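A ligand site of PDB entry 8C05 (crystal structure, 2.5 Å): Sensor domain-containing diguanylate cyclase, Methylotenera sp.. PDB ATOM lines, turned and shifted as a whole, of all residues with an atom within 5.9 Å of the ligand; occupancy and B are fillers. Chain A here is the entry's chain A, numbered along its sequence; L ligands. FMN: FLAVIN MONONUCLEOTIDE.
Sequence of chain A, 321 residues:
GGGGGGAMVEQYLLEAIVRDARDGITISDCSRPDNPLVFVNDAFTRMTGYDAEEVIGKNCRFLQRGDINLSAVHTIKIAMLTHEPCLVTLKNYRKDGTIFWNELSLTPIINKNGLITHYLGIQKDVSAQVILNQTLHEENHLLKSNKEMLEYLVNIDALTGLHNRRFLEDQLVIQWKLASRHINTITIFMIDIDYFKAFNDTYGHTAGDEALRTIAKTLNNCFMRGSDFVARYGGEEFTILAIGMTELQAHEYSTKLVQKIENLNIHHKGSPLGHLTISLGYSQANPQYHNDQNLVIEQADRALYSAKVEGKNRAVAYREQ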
ATOM      1  N   THR A  26       9.533  -1.490 -12.121  1.00  0.00           N
ATOM      2  CA  THR A  26       8.816  -0.423 -12.808  1.00  0.00           C
ATOM      3  C   THR A  26       9.684   0.837 -12.843  1.00  0.00           C
ATOM      4  O   THR A  26      10.445   1.111 -11.909  1.00  0.00           O
ATOM      5  CB  THR A  26       7.478  -0.104 -12.132  1.00  0.00           C
ATOM      6  OG1 THR A  26       7.697   0.189 -10.745  1.00  0.00           O
ATOM      7  CG2 THR A  26       6.525  -1.277 -12.252  1.00  0.00           C
ATOM      8  N   ILE A  27       9.544   1.586 -13.931  1.00  0.00           N
ATOM      9  CA  ILE A  27      10.212   2.877 -14.108  1.00  0.00           C
ATOM     10  C   ILE A  27       9.139   3.906 -14.407  1.00  0.00           C
ATOM     11  O   ILE A  27       8.293   3.696 -15.276  1.00  0.00           O
ATOM     12  CB  ILE A  27      11.265   2.828 -15.224  1.00  0.00           C
ATOM     13  CG1 ILE A  27      12.299   1.739 -14.955  1.00  0.00           C
ATOM     14  CG2 ILE A  27      11.947   4.179 -15.375  1.00  0.00           C
ATOM     15  CD1 ILE A  27      13.144   2.010 -13.733  1.00  0.00           C
ATOM     16  N   SER A  28       9.185   5.022 -13.685  1.00  0.00           N
ATOM     17  CA  SER A  28       8.202   6.088 -13.840  1.00  0.00           C
ATOM     18  C   SER A  28       8.902   7.399 -14.168  1.00  0.00           C
ATOM     19  O   SER A  28       9.928   7.729 -13.566  1.00  0.00           O
ATOM     20  CB  SER A  28       7.368   6.261 -12.560  1.00  0.00           C
ATOM     21  OG  SER A  28       8.190   6.624 -11.469  1.00  0.00           O
ATOM     22  N   ASP A  34       2.100  13.544 -12.129  1.00  0.00           N
ATOM     23  CA  ASP A  34       1.538  12.339 -11.510  1.00  0.00           C
ATOM     24  C   ASP A  34       2.471  11.136 -11.610  1.00  0.00           C
ATOM     25  O   ASP A  34       2.090  10.037 -11.196  1.00  0.00           O
ATOM     26  CB  ASP A  34       0.172  11.983 -12.100  1.00  0.00           C
ATOM     27  CG  ASP A  34      -0.683  11.172 -11.134  1.00  0.00           C
ATOM     28  OD1 ASP A  34      -0.266  10.990  -9.978  1.00  0.00           O
ATOM     29  OD2 ASP A  34      -1.776  10.723 -11.550  1.00  0.00           O
ATOM     30  N   ASN A  35       3.686  11.319 -12.136  1.00  0.00           N
ATOM     31  CA  ASN A  35       4.697  10.269 -12.256  1.00  0.00           C
ATOM     32  C   ASN A  35       4.143   9.049 -12.981  1.00  0.00           C
ATOM     33  O   ASN A  35       3.914   8.004 -12.360  1.00  0.00           O
ATOM     34  CB  ASN A  35       5.213   9.871 -10.863  1.00  0.00           C
ATOM     35  CG  ASN A  35       5.563  11.077 -10.021  1.00  0.00           C
ATOM     36  OD1 ASN A  35       6.653  11.636 -10.132  1.00  0.00           O
ATOM     37  ND2 ASN A  35       4.641  11.482  -9.149  1.00  0.00           N
ATOM     38  N   LEU A  37       3.895   5.636 -15.180  1.00  0.00           N
ATOM     39  CA  LEU A  37       4.756   4.480 -15.394  1.00  0.00           C
ATOM     40  C   LEU A  37       5.228   4.430 -16.840  1.00  0.00           C
ATOM     41  O   LEU A  37       4.405   4.388 -17.764  1.00  0.00           O
ATOM     42  CB  LEU A  37       4.013   3.203 -15.019  1.00  0.00           C
ATOM     43  CG  LEU A  37       3.653   3.003 -13.541  1.00  0.00           C
ATOM     44  CD1 LEU A  37       2.733   1.806 -13.357  1.00  0.00           C
ATOM     45  CD2 LEU A  37       4.918   2.844 -12.706  1.00  0.00           C
ATOM     46  N   PHE A  44       6.215  -7.834 -13.128  1.00  0.00           N
ATOM     47  CA  PHE A  44       5.130  -6.969 -12.670  1.00  0.00           C
ATOM     48  C   PHE A  44       3.786  -7.457 -13.201  1.00  0.00           C
ATOM     49  O   PHE A  44       2.810  -7.568 -12.444  1.00  0.00           O
ATOM     50  CB  PHE A  44       5.389  -5.526 -13.089  1.00  0.00           C
ATOM     51  CG  PHE A  44       4.326  -4.554 -12.640  1.00  0.00           C
ATOM     52  CD1 PHE A  44       4.371  -3.998 -11.372  1.00  0.00           C
ATOM     53  CD2 PHE A  44       3.285  -4.200 -13.478  1.00  0.00           C
ATOM     54  CE1 PHE A  44       3.401  -3.108 -10.948  1.00  0.00           C
ATOM     55  CE2 PHE A  44       2.308  -3.312 -13.061  1.00  0.00           C
ATOM     56  CZ  PHE A  44       2.368  -2.768 -11.804  1.00  0.00           C
ATOM     57  N   ASN A  59      -0.420   6.279 -13.399  1.00  0.00           N
ATOM     58  CA  ASN A  59       0.119   6.163 -12.053  1.00  0.00           C
ATOM     59  C   ASN A  59      -0.222   4.807 -11.463  1.00  0.00           C
ATOM     60  O   ASN A  59      -1.321   4.289 -11.669  1.00  0.00           O
ATOM     61  CB  ASN A  59      -0.428   7.285 -11.165  1.00  0.00           C
ATOM     62  CG  ASN A  59       0.216   7.300  -9.788  1.00  0.00           C
ATOM     63  OD1 ASN A  59      -0.239   6.615  -8.863  1.00  0.00           O
ATOM     64  ND2 ASN A  59       1.278   8.080  -9.634  1.00  0.00           N
ATOM     65  N   CYS A  60       0.726   4.229 -10.728  1.00  0.00           N
ATOM     66  CA  CYS A  60       0.570   2.876 -10.206  1.00  0.00           C
ATOM     67  C   CYS A  60      -0.415   2.782  -9.031  1.00  0.00           C
ATOM     68  O   CYS A  60      -0.446   1.741  -8.363  1.00  0.00           O
ATOM     69  CB  CYS A  60       1.934   2.327  -9.785  1.00  0.00           C
ATOM     70  SG  CYS A  60       2.060   0.519  -9.810  1.00  0.00           S
ATOM     71  N   ARG A  61      -1.221   3.806  -8.733  1.00  0.00           N
ATOM     72  CA  ARG A  61      -2.159   3.732  -7.624  1.00  0.00           C
ATOM     73  C   ARG A  61      -3.354   2.832  -7.912  1.00  0.00           C
ATOM     74  O   ARG A  61      -4.172   2.619  -7.009  1.00  0.00           O
ATOM     75  CB  ARG A  61      -2.655   5.130  -7.250  1.00  0.00           C
ATOM     76  CG  ARG A  61      -3.399   5.848  -8.367  1.00  0.00           C
ATOM     77  CD  ARG A  61      -3.955   7.174  -7.886  1.00  0.00           C
ATOM     78  NE  ARG A  61      -2.918   8.032  -7.316  1.00  0.00           N
ATOM     79  CZ  ARG A  61      -2.243   8.942  -8.006  1.00  0.00           C
ATOM     80  NH1 ARG A  61      -2.473   9.153  -9.282  1.00  0.00           N
ATOM     81  NH2 ARG A  61      -1.309   9.661  -7.382  1.00  0.00           N
ATOM     82  N   LEU A  63      -3.321  -0.232  -8.074  1.00  0.00           N
ATOM     83  CA  LEU A  63      -3.204  -1.404  -7.215  1.00  0.00           C
ATOM     84  C   LEU A  63      -3.792  -1.167  -5.836  1.00  0.00           C
ATOM     85  O   LEU A  63      -4.086  -2.141  -5.130  1.00  0.00           O
ATOM     86  CB  LEU A  63      -1.729  -1.806  -7.087  1.00  0.00           C
ATOM     87  CG  LEU A  63      -1.015  -2.158  -8.385  1.00  0.00           C
ATOM     88  CD1 LEU A  63       0.454  -2.419  -8.133  1.00  0.00           C
ATOM     89  CD2 LEU A  63      -1.666  -3.362  -9.061  1.00  0.00           C
ATOM     90  N   GLN A  64      -3.991   0.084  -5.440  1.00  0.00           N
ATOM     91  CA  GLN A  64      -4.501   0.415  -4.122  1.00  0.00           C
ATOM     92  C   GLN A  64      -6.019   0.494  -4.131  1.00  0.00           C
ATOM     93  O   GLN A  64      -6.658   0.722  -5.170  1.00  0.00           O
ATOM     94  CB  GLN A  64      -3.917   1.750  -3.645  1.00  0.00           C
ATOM     95  CG  GLN A  64      -2.397   1.784  -3.614  1.00  0.00           C
ATOM     96  CD  GLN A  64      -1.857   3.195  -3.486  1.00  0.00           C
ATOM     97  OE1 GLN A  64      -2.578   4.167  -3.670  1.00  0.00           O
ATOM     98  NE2 GLN A  64      -0.576   3.302  -3.157  1.00  0.00           N
ATOM     99  N   ILE A  68      -6.142   0.615   1.919  1.00  0.00           N
ATOM    100  CA  ILE A  68      -4.701   0.794   1.944  1.00  0.00           C
ATOM    101  C   ILE A  68      -4.291   1.597   3.170  1.00  0.00           C
ATOM    102  O   ILE A  68      -5.057   2.437   3.681  1.00  0.00           O
ATOM    103  CB  ILE A  68      -4.226   1.469   0.646  1.00  0.00           C
ATOM    104  CG1 ILE A  68      -2.704   1.374   0.498  1.00  0.00           C
ATOM    105  CG2 ILE A  68      -4.685   2.916   0.584  1.00  0.00           C
ATOM    106  CD1 ILE A  68      -2.193  -0.047   0.430  1.00  0.00           C
ATOM    107  N   VAL A  73       0.990   5.310   2.220  1.00  0.00           N
ATOM    108  CA  VAL A  73       0.832   6.096   0.996  1.00  0.00           C
ATOM    109  C   VAL A  73       1.295   7.526   1.207  1.00  0.00           C
ATOM    110  O   VAL A  73       1.859   8.160   0.305  1.00  0.00           O
ATOM    111  CB  VAL A  73      -0.626   6.036   0.512  1.00  0.00           C
ATOM    112  CG1 VAL A  73      -0.774   6.762  -0.819  1.00  0.00           C
ATOM    113  CG2 VAL A  73      -1.087   4.598   0.386  1.00  0.00           C
ATOM    114  N   HIS A  74       1.075   8.068   2.411  1.00  0.00           N
ATOM    115  CA  HIS A  74       1.546   9.409   2.712  1.00  0.00           C
ATOM    116  C   HIS A  74       3.067   9.457   2.738  1.00  0.00           C
ATOM    117  O   HIS A  74       3.671  10.458   2.320  1.00  0.00           O
ATOM    118  CB  HIS A  74       0.953   9.891   4.039  1.00  0.00           C
ATOM    119  CG  HIS A  74       1.157  11.353   4.295  1.00  0.00           C
ATOM    120  ND1 HIS A  74       0.693  12.333   3.444  1.00  0.00           N
ATOM    121  CD2 HIS A  74       1.761  11.999   5.319  1.00  0.00           C
ATOM    122  CE1 HIS A  74       1.012  13.517   3.937  1.00  0.00           C
ATOM    123  NE2 HIS A  74       1.656  13.350   5.068  1.00  0.00           N
ATOM    124  N   ILE A  76       4.985   7.553   0.904  1.00  0.00           N
ATOM    125  CA  ILE A  76       5.363   7.526  -0.514  1.00  0.00           C
ATOM    126  C   ILE A  76       5.306   8.931  -1.100  1.00  0.00           C
ATOM    127  O   ILE A  76       6.240   9.382  -1.769  1.00  0.00           O
ATOM    128  CB  ILE A  76       4.455   6.558  -1.292  1.00  0.00           C
ATOM    129  CG1 ILE A  76       4.685   5.119  -0.838  1.00  0.00           C
ATOM    130  CG2 ILE A  76       4.684   6.702  -2.785  1.00  0.00           C
ATOM    131  CD1 ILE A  76       3.790   4.125  -1.536  1.00  0.00           C
ATOM    132  N   LYS A  77       4.205   9.642  -0.852  1.00  0.00           N
ATOM    133  CA  LYS A  77       4.023  10.966  -1.436  1.00  0.00           C
ATOM    134  C   LYS A  77       5.076  11.943  -0.930  1.00  0.00           C
ATOM    135  O   LYS A  77       5.644  12.714  -1.718  1.00  0.00           O
ATOM    136  CB  LYS A  77       2.616  11.482  -1.134  1.00  0.00           C
ATOM    137  CG  LYS A  77       2.242  12.764  -1.874  1.00  0.00           C
ATOM    138  CD  LYS A  77       1.011  13.404  -1.267  1.00  0.00           C
ATOM    139  CE  LYS A  77      -0.148  12.425  -1.169  1.00  0.00           C
ATOM    140  NZ  LYS A  77      -1.321  13.017  -0.475  1.00  0.00           N
ATOM    141  N   MET A  80       8.555  11.142  -2.476  1.00  0.00           N
ATOM    142  CA  MET A  80       8.686  11.535  -3.872  1.00  0.00           C
ATOM    143  C   MET A  80       8.791  13.045  -4.017  1.00  0.00           C
ATOM    144  O   MET A  80       9.518  13.541  -4.898  1.00  0.00           O
ATOM    145  CB  MET A  80       7.510  11.000  -4.683  1.00  0.00           C
ATOM    146  CG  MET A  80       7.419   9.486  -4.721  1.00  0.00           C
ATOM    147  SD  MET A  80       6.323   8.910  -6.025  1.00  0.00           S
ATOM    148  CE  MET A  80       7.208   9.518  -7.463  1.00  0.00           C
ATOM    149  N   LEU A  90       2.597  -2.501   1.366  1.00  0.00           N
ATOM    150  CA  LEU A  90       1.269  -2.077   0.961  1.00  0.00           C
ATOM    151  C   LEU A  90       0.396  -3.288   0.659  1.00  0.00           C
ATOM    152  O   LEU A  90       0.883  -4.359   0.316  1.00  0.00           O
ATOM    153  CB  LEU A  90       1.343  -1.170  -0.282  1.00  0.00           C
ATOM    154  CG  LEU A  90       2.198   0.091  -0.120  1.00  0.00           C
ATOM    155  CD1 LEU A  90       2.723   0.559  -1.465  1.00  0.00           C
ATOM    156  CD2 LEU A  90       1.395   1.185   0.554  1.00  0.00           C
ATOM    157  N   ASN A  92      -1.996  -4.446  -1.940  1.00  0.00           N
ATOM    158  CA  ASN A  92      -2.394  -4.176  -3.311  1.00  0.00           C
ATOM    159  C   ASN A  92      -3.335  -5.253  -3.826  1.00  0.00           C
ATOM    160  O   ASN A  92      -3.351  -6.390  -3.345  1.00  0.00           O
ATOM    161  CB  ASN A  92      -1.168  -4.075  -4.224  1.00  0.00           C
ATOM    162  CG  ASN A  92      -0.295  -2.880  -3.904  1.00  0.00           C
ATOM    163  OD1 ASN A  92       0.926  -2.912  -4.075  1.00  0.00           O
ATOM    164  ND2 ASN A  92      -0.918  -1.800  -3.430  1.00  0.00           N
ATOM    165  N   ASN A 102       2.585  -6.196  -0.869  1.00  0.00           N
ATOM    166  CA  ASN A 102       3.665  -5.685  -1.685  1.00  0.00           C
ATOM    167  C   ASN A 102       4.605  -4.836  -0.833  1.00  0.00           C
ATOM    168  O   ASN A 102       4.183  -3.816  -0.282  1.00  0.00           O
ATOM    169  CB  ASN A 102       3.119  -4.870  -2.853  1.00  0.00           C
ATOM    170  CG  ASN A 102       4.203  -4.174  -3.653  1.00  0.00           C
ATOM    171  OD1 ASN A 102       5.359  -4.608  -3.676  1.00  0.00           O
ATOM    172  ND2 ASN A 102       3.840  -3.089  -4.333  1.00  0.00           N
ATOM    173  N   LEU A 104       7.133  -2.381  -1.418  1.00  0.00           N
ATOM    174  CA  LEU A 104       7.550  -1.530  -2.523  1.00  0.00           C
ATOM    175  C   LEU A 104       8.747  -0.681  -2.122  1.00  0.00           C
ATOM    176  O   LEU A 104       8.702   0.018  -1.106  1.00  0.00           O
ATOM    177  CB  LEU A 104       6.404  -0.628  -2.986  1.00  0.00           C
ATOM    178  CG  LEU A 104       6.787   0.430  -4.017  1.00  0.00           C
ATOM    179  CD1 LEU A 104       7.128  -0.211  -5.353  1.00  0.00           C
ATOM    180  CD2 LEU A 104       5.691   1.467  -4.167  1.00  0.00           C
ATOM    181  N   LEU A 106      10.972   2.385  -3.468  1.00  0.00           N
ATOM    182  CA  LEU A 106      11.123   3.481  -4.412  1.00  0.00           C
ATOM    183  C   LEU A 106      12.504   4.104  -4.240  1.00  0.00           C
ATOM    184  O   LEU A 106      12.983   4.282  -3.119  1.00  0.00           O
ATOM    185  CB  LEU A 106      10.041   4.538  -4.197  1.00  0.00           C
ATOM    186  CG  LEU A 106       8.615   4.107  -4.535  1.00  0.00           C
ATOM    187  CD1 LEU A 106       7.638   5.238  -4.286  1.00  0.00           C
ATOM    188  CD2 LEU A 106       8.527   3.621  -5.981  1.00  0.00           C
ATOM    189  N   TYR A 119      11.986   7.331 -11.456  1.00  0.00           N
ATOM    190  CA  TYR A 119      11.859   6.652 -10.169  1.00  0.00           C
ATOM    191  C   TYR A 119      11.806   5.150 -10.404  1.00  0.00           C
ATOM    192  O   TYR A 119      11.175   4.682 -11.353  1.00  0.00           O
ATOM    193  CB  TYR A 119      10.610   7.115  -9.407  1.00  0.00           C
ATOM    194  CG  TYR A 119      10.900   7.750  -8.059  1.00  0.00           C
ATOM    195  CD1 TYR A 119      11.079   9.129  -7.941  1.00  0.00           C
ATOM    196  CD2 TYR A 119      10.977   6.983  -6.903  1.00  0.00           C
ATOM    197  CE1 TYR A 119      11.338   9.708  -6.717  1.00  0.00           C
ATOM    198  CE2 TYR A 119      11.230   7.558  -5.673  1.00  0.00           C
ATOM    199  CZ  TYR A 119      11.416   8.925  -5.586  1.00  0.00           C
ATOM    200  OH  TYR A 119      11.674   9.504  -4.362  1.00  0.00           O
ATOM    201  N   LEU A 120      12.471   4.392  -9.526  1.00  0.00           N
ATOM    202  CA  LEU A 120      12.538   2.945  -9.624  1.00  0.00           C
ATOM    203  C   LEU A 120      11.618   2.324  -8.577  1.00  0.00           C
ATOM    204  O   LEU A 120      11.781   2.577  -7.382  1.00  0.00           O
ATOM    205  CB  LEU A 120      13.969   2.443  -9.425  1.00  0.00           C
ATOM    206  CG  LEU A 120      14.114   0.921  -9.335  1.00  0.00           C
ATOM    207  CD1 LEU A 120      13.637   0.273 -10.625  1.00  0.00           C
ATOM    208  CD2 LEU A 120      15.544   0.508  -9.031  1.00  0.00           C
ATOM    209  N   GLY A 121      10.670   1.507  -9.031  1.00  0.00           N
ATOM    210  CA  GLY A 121       9.768   0.828  -8.128  1.00  0.00           C
ATOM    211  C   GLY A 121       9.903  -0.686  -8.188  1.00  0.00           C
ATOM    212  O   GLY A 121       9.576  -1.309  -9.204  1.00  0.00           O
ATOM    213  N   GLN A 123       8.648  -4.128  -6.712  1.00  0.00           N
ATOM    214  CA  GLN A 123       7.556  -4.764  -5.978  1.00  0.00           C
ATOM    215  C   GLN A 123       7.942  -6.203  -5.648  1.00  0.00           C
ATOM    216  O   GLN A 123       8.314  -6.974  -6.549  1.00  0.00           O
ATOM    217  CB  GLN A 123       6.268  -4.740  -6.795  1.00  0.00           C
ATOM    218  CG  GLN A 123       5.750  -3.341  -7.114  1.00  0.00           C
ATOM    219  CD  GLN A 123       6.438  -2.717  -8.305  1.00  0.00           C
ATOM    220  OE1 GLN A 123       7.259  -3.358  -8.969  1.00  0.00           O
ATOM    221  NE2 GLN A 123       6.120  -1.462  -8.593  1.00  0.00           N
HETATM  222  N1  FMN L   1       1.902   2.000  -5.038  1.00  0.00           N
HETATM  223  C2  FMN L   1       1.404   0.762  -4.699  1.00  0.00           C
HETATM  224  O2  FMN L   1       0.546   0.652  -3.829  1.00  0.00           O
HETATM  225  N3  FMN L   1       1.860  -0.377  -5.350  1.00  0.00           N
HETATM  226  C4  FMN L   1       2.816  -0.267  -6.330  1.00  0.00           C
HETATM  227  O4  FMN L   1       3.243  -1.282  -6.888  1.00  0.00           O
HETATM  228  C4A FMN L   1       3.320   0.976  -6.676  1.00  0.00           C
HETATM  229  N5  FMN L   1       4.308   1.085  -7.630  1.00  0.00           N
HETATM  230  C5A FMN L   1       4.896   2.303  -7.879  1.00  0.00           C
HETATM  231  C6  FMN L   1       5.965   2.380  -8.761  1.00  0.00           C
HETATM  232  C7  FMN L   1       6.579   3.609  -8.996  1.00  0.00           C
HETATM  233  C7M FMN L   1       7.740   3.684  -9.952  1.00  0.00           C
HETATM  234  C8  FMN L   1       6.116   4.745  -8.352  1.00  0.00           C
HETATM  235  C8M FMN L   1       6.773   6.074  -8.615  1.00  0.00           C
HETATM  236  C9  FMN L   1       5.047   4.668  -7.471  1.00  0.00           C
HETATM  237  C9A FMN L   1       4.440   3.442  -7.228  1.00  0.00           C
HETATM  238  N10 FMN L   1       3.375   3.356  -6.349  1.00  0.00           N
HETATM  239  C10 FMN L   1       2.863   2.114  -6.025  1.00  0.00           C
HETATM  240  C1' FMN L   1       2.902   4.583  -5.621  1.00  0.00           C
HETATM  241  C2' FMN L   1       1.668   5.166  -6.307  1.00  0.00           C
HETATM  242  O2' FMN L   1       1.843   5.128  -7.708  1.00  0.00           O
HETATM  243  C3' FMN L   1       1.418   6.597  -5.855  1.00  0.00           C
HETATM  244  O3' FMN L   1       2.462   7.430  -6.312  1.00  0.00           O
HETATM  245  C4' FMN L   1       1.320   6.684  -4.342  1.00  0.00           C
HETATM  246  O4' FMN L   1       0.235   5.913  -3.890  1.00  0.00           O
HETATM  247  C5' FMN L   1       1.136   8.128  -3.887  1.00  0.00           C
HETATM  248  O5' FMN L   1       0.153   8.758  -4.674  1.00  0.00           O
HETATM  249  P   FMN L   1      -1.234   9.253  -4.016  1.00  0.00           P
HETATM  250  O1P FMN L   1      -1.010   9.595  -2.576  1.00  0.00           O
HETATM  251  O2P FMN L   1      -1.731  10.467  -4.759  1.00  0.00           O
HETATM  252  O3P FMN L   1      -2.261   8.142  -4.124  1.00  0.00           O
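An oxygen (O2') of the ligand is in hydrogen-bond range of the backbone NH of Arg 61. The guanidinium group (NH2) of Arg 61 lies within salt-bridge range of an oxygen (O2P) of the ligand (2.8 Å). An oxygen (O2') of the ligand sits at hydrogen-bond distance from the side-chain amide oxygen (OD1) of Asn 59, at 2.8 Å. NE2 of Gln 64 sits at hydrogen-bond distance from O4' of the ligand. O2 of the ligand sits at hydrogen-bond distance from ND2 of Asn 92. N of Cys 60 lies within hydrogen-bond range of O2' of the ligand (3.3 Å). The side-chain sulfur (SG) of Cys 60 is in hydrogen-bond range of a nitrogen (N5) of the ligand (3.2 Å). ND2 of Asn 102 lies within hydrogen-bond range of O4 of the ligand, at 3.2 Å. The side-chain amide nitrogen (NE2) of Gln 123 lies within hydrogen-bond range of a nitrogen (N5) of the ligand (3.3 Å).
Thr 26 touches the ligand (OG1 to C6, 3.4 Å). Ser 28 touches the ligand. Leu 63 touches the ligand. Val 73 touches the ligand. Ile 76 touches the ligand (CG2 to C4', 3.7 Å). Lys 77 touches the ligand (CE to O1P, 3.3 Å). Met 80 touches the ligand. Leu 90 touches the ligand (CD1 to O2, 3.2 Å). CD2 of Leu 104 touches C10 of the ligand, at 3.4 Å. CD2 of Leu 106 touches C8 of the ligand, at 3.6 Å. O of Tyr 119 touches C7M of the ligand (3.8 Å). N of Gly 121 touches C7M of the ligand, 3.8 Å away. Hydrophobic or aromatic side chains that line the ligand: Leu 63, Val 73, Ile 76, Met 80, Leu 90, Leu 104 and Leu 106. The nearest printed residue that does not touch the ligand is Leu 37 (4.03 Å).
The backbone NH (N) of Arg 61 lies within hydrogen-bond range of the side-chain amide oxygen (OD1) of Asn 59, at 3.0 Å. The side-chain carboxylate of Asp 34 lies within salt-bridge range of the guanidinium group of Arg 61 (2.8 Å). The backbone carbonyl oxygen of Asp 34 is in hydrogen-bond range of the side-chain amide nitrogen of Asn 59 (2.6 Å). ND2 of Asn 102 lies within hydrogen-bond range of OD1 of Asn 92, at 2.9 Å. The backbone carbonyl oxygen (O) of Asn 102 sits at hydrogen-bond distance from the backbone NH (N) of Leu 90. The side-chain amide nitrogen (NE2) of Gln 123 is in hydrogen-bond range of the side-chain hydroxyl (OG1) of Thr 26. The backbone carbonyl oxygen of Gly 121 lies close to the side-chain amide oxygen of Gln 123 (3.1 Å). The side-chain hydroxyl of Thr 26 sits at hydrogen-bond distance from the backbone carbonyl oxygen of Gly 121 (2.9 Å).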
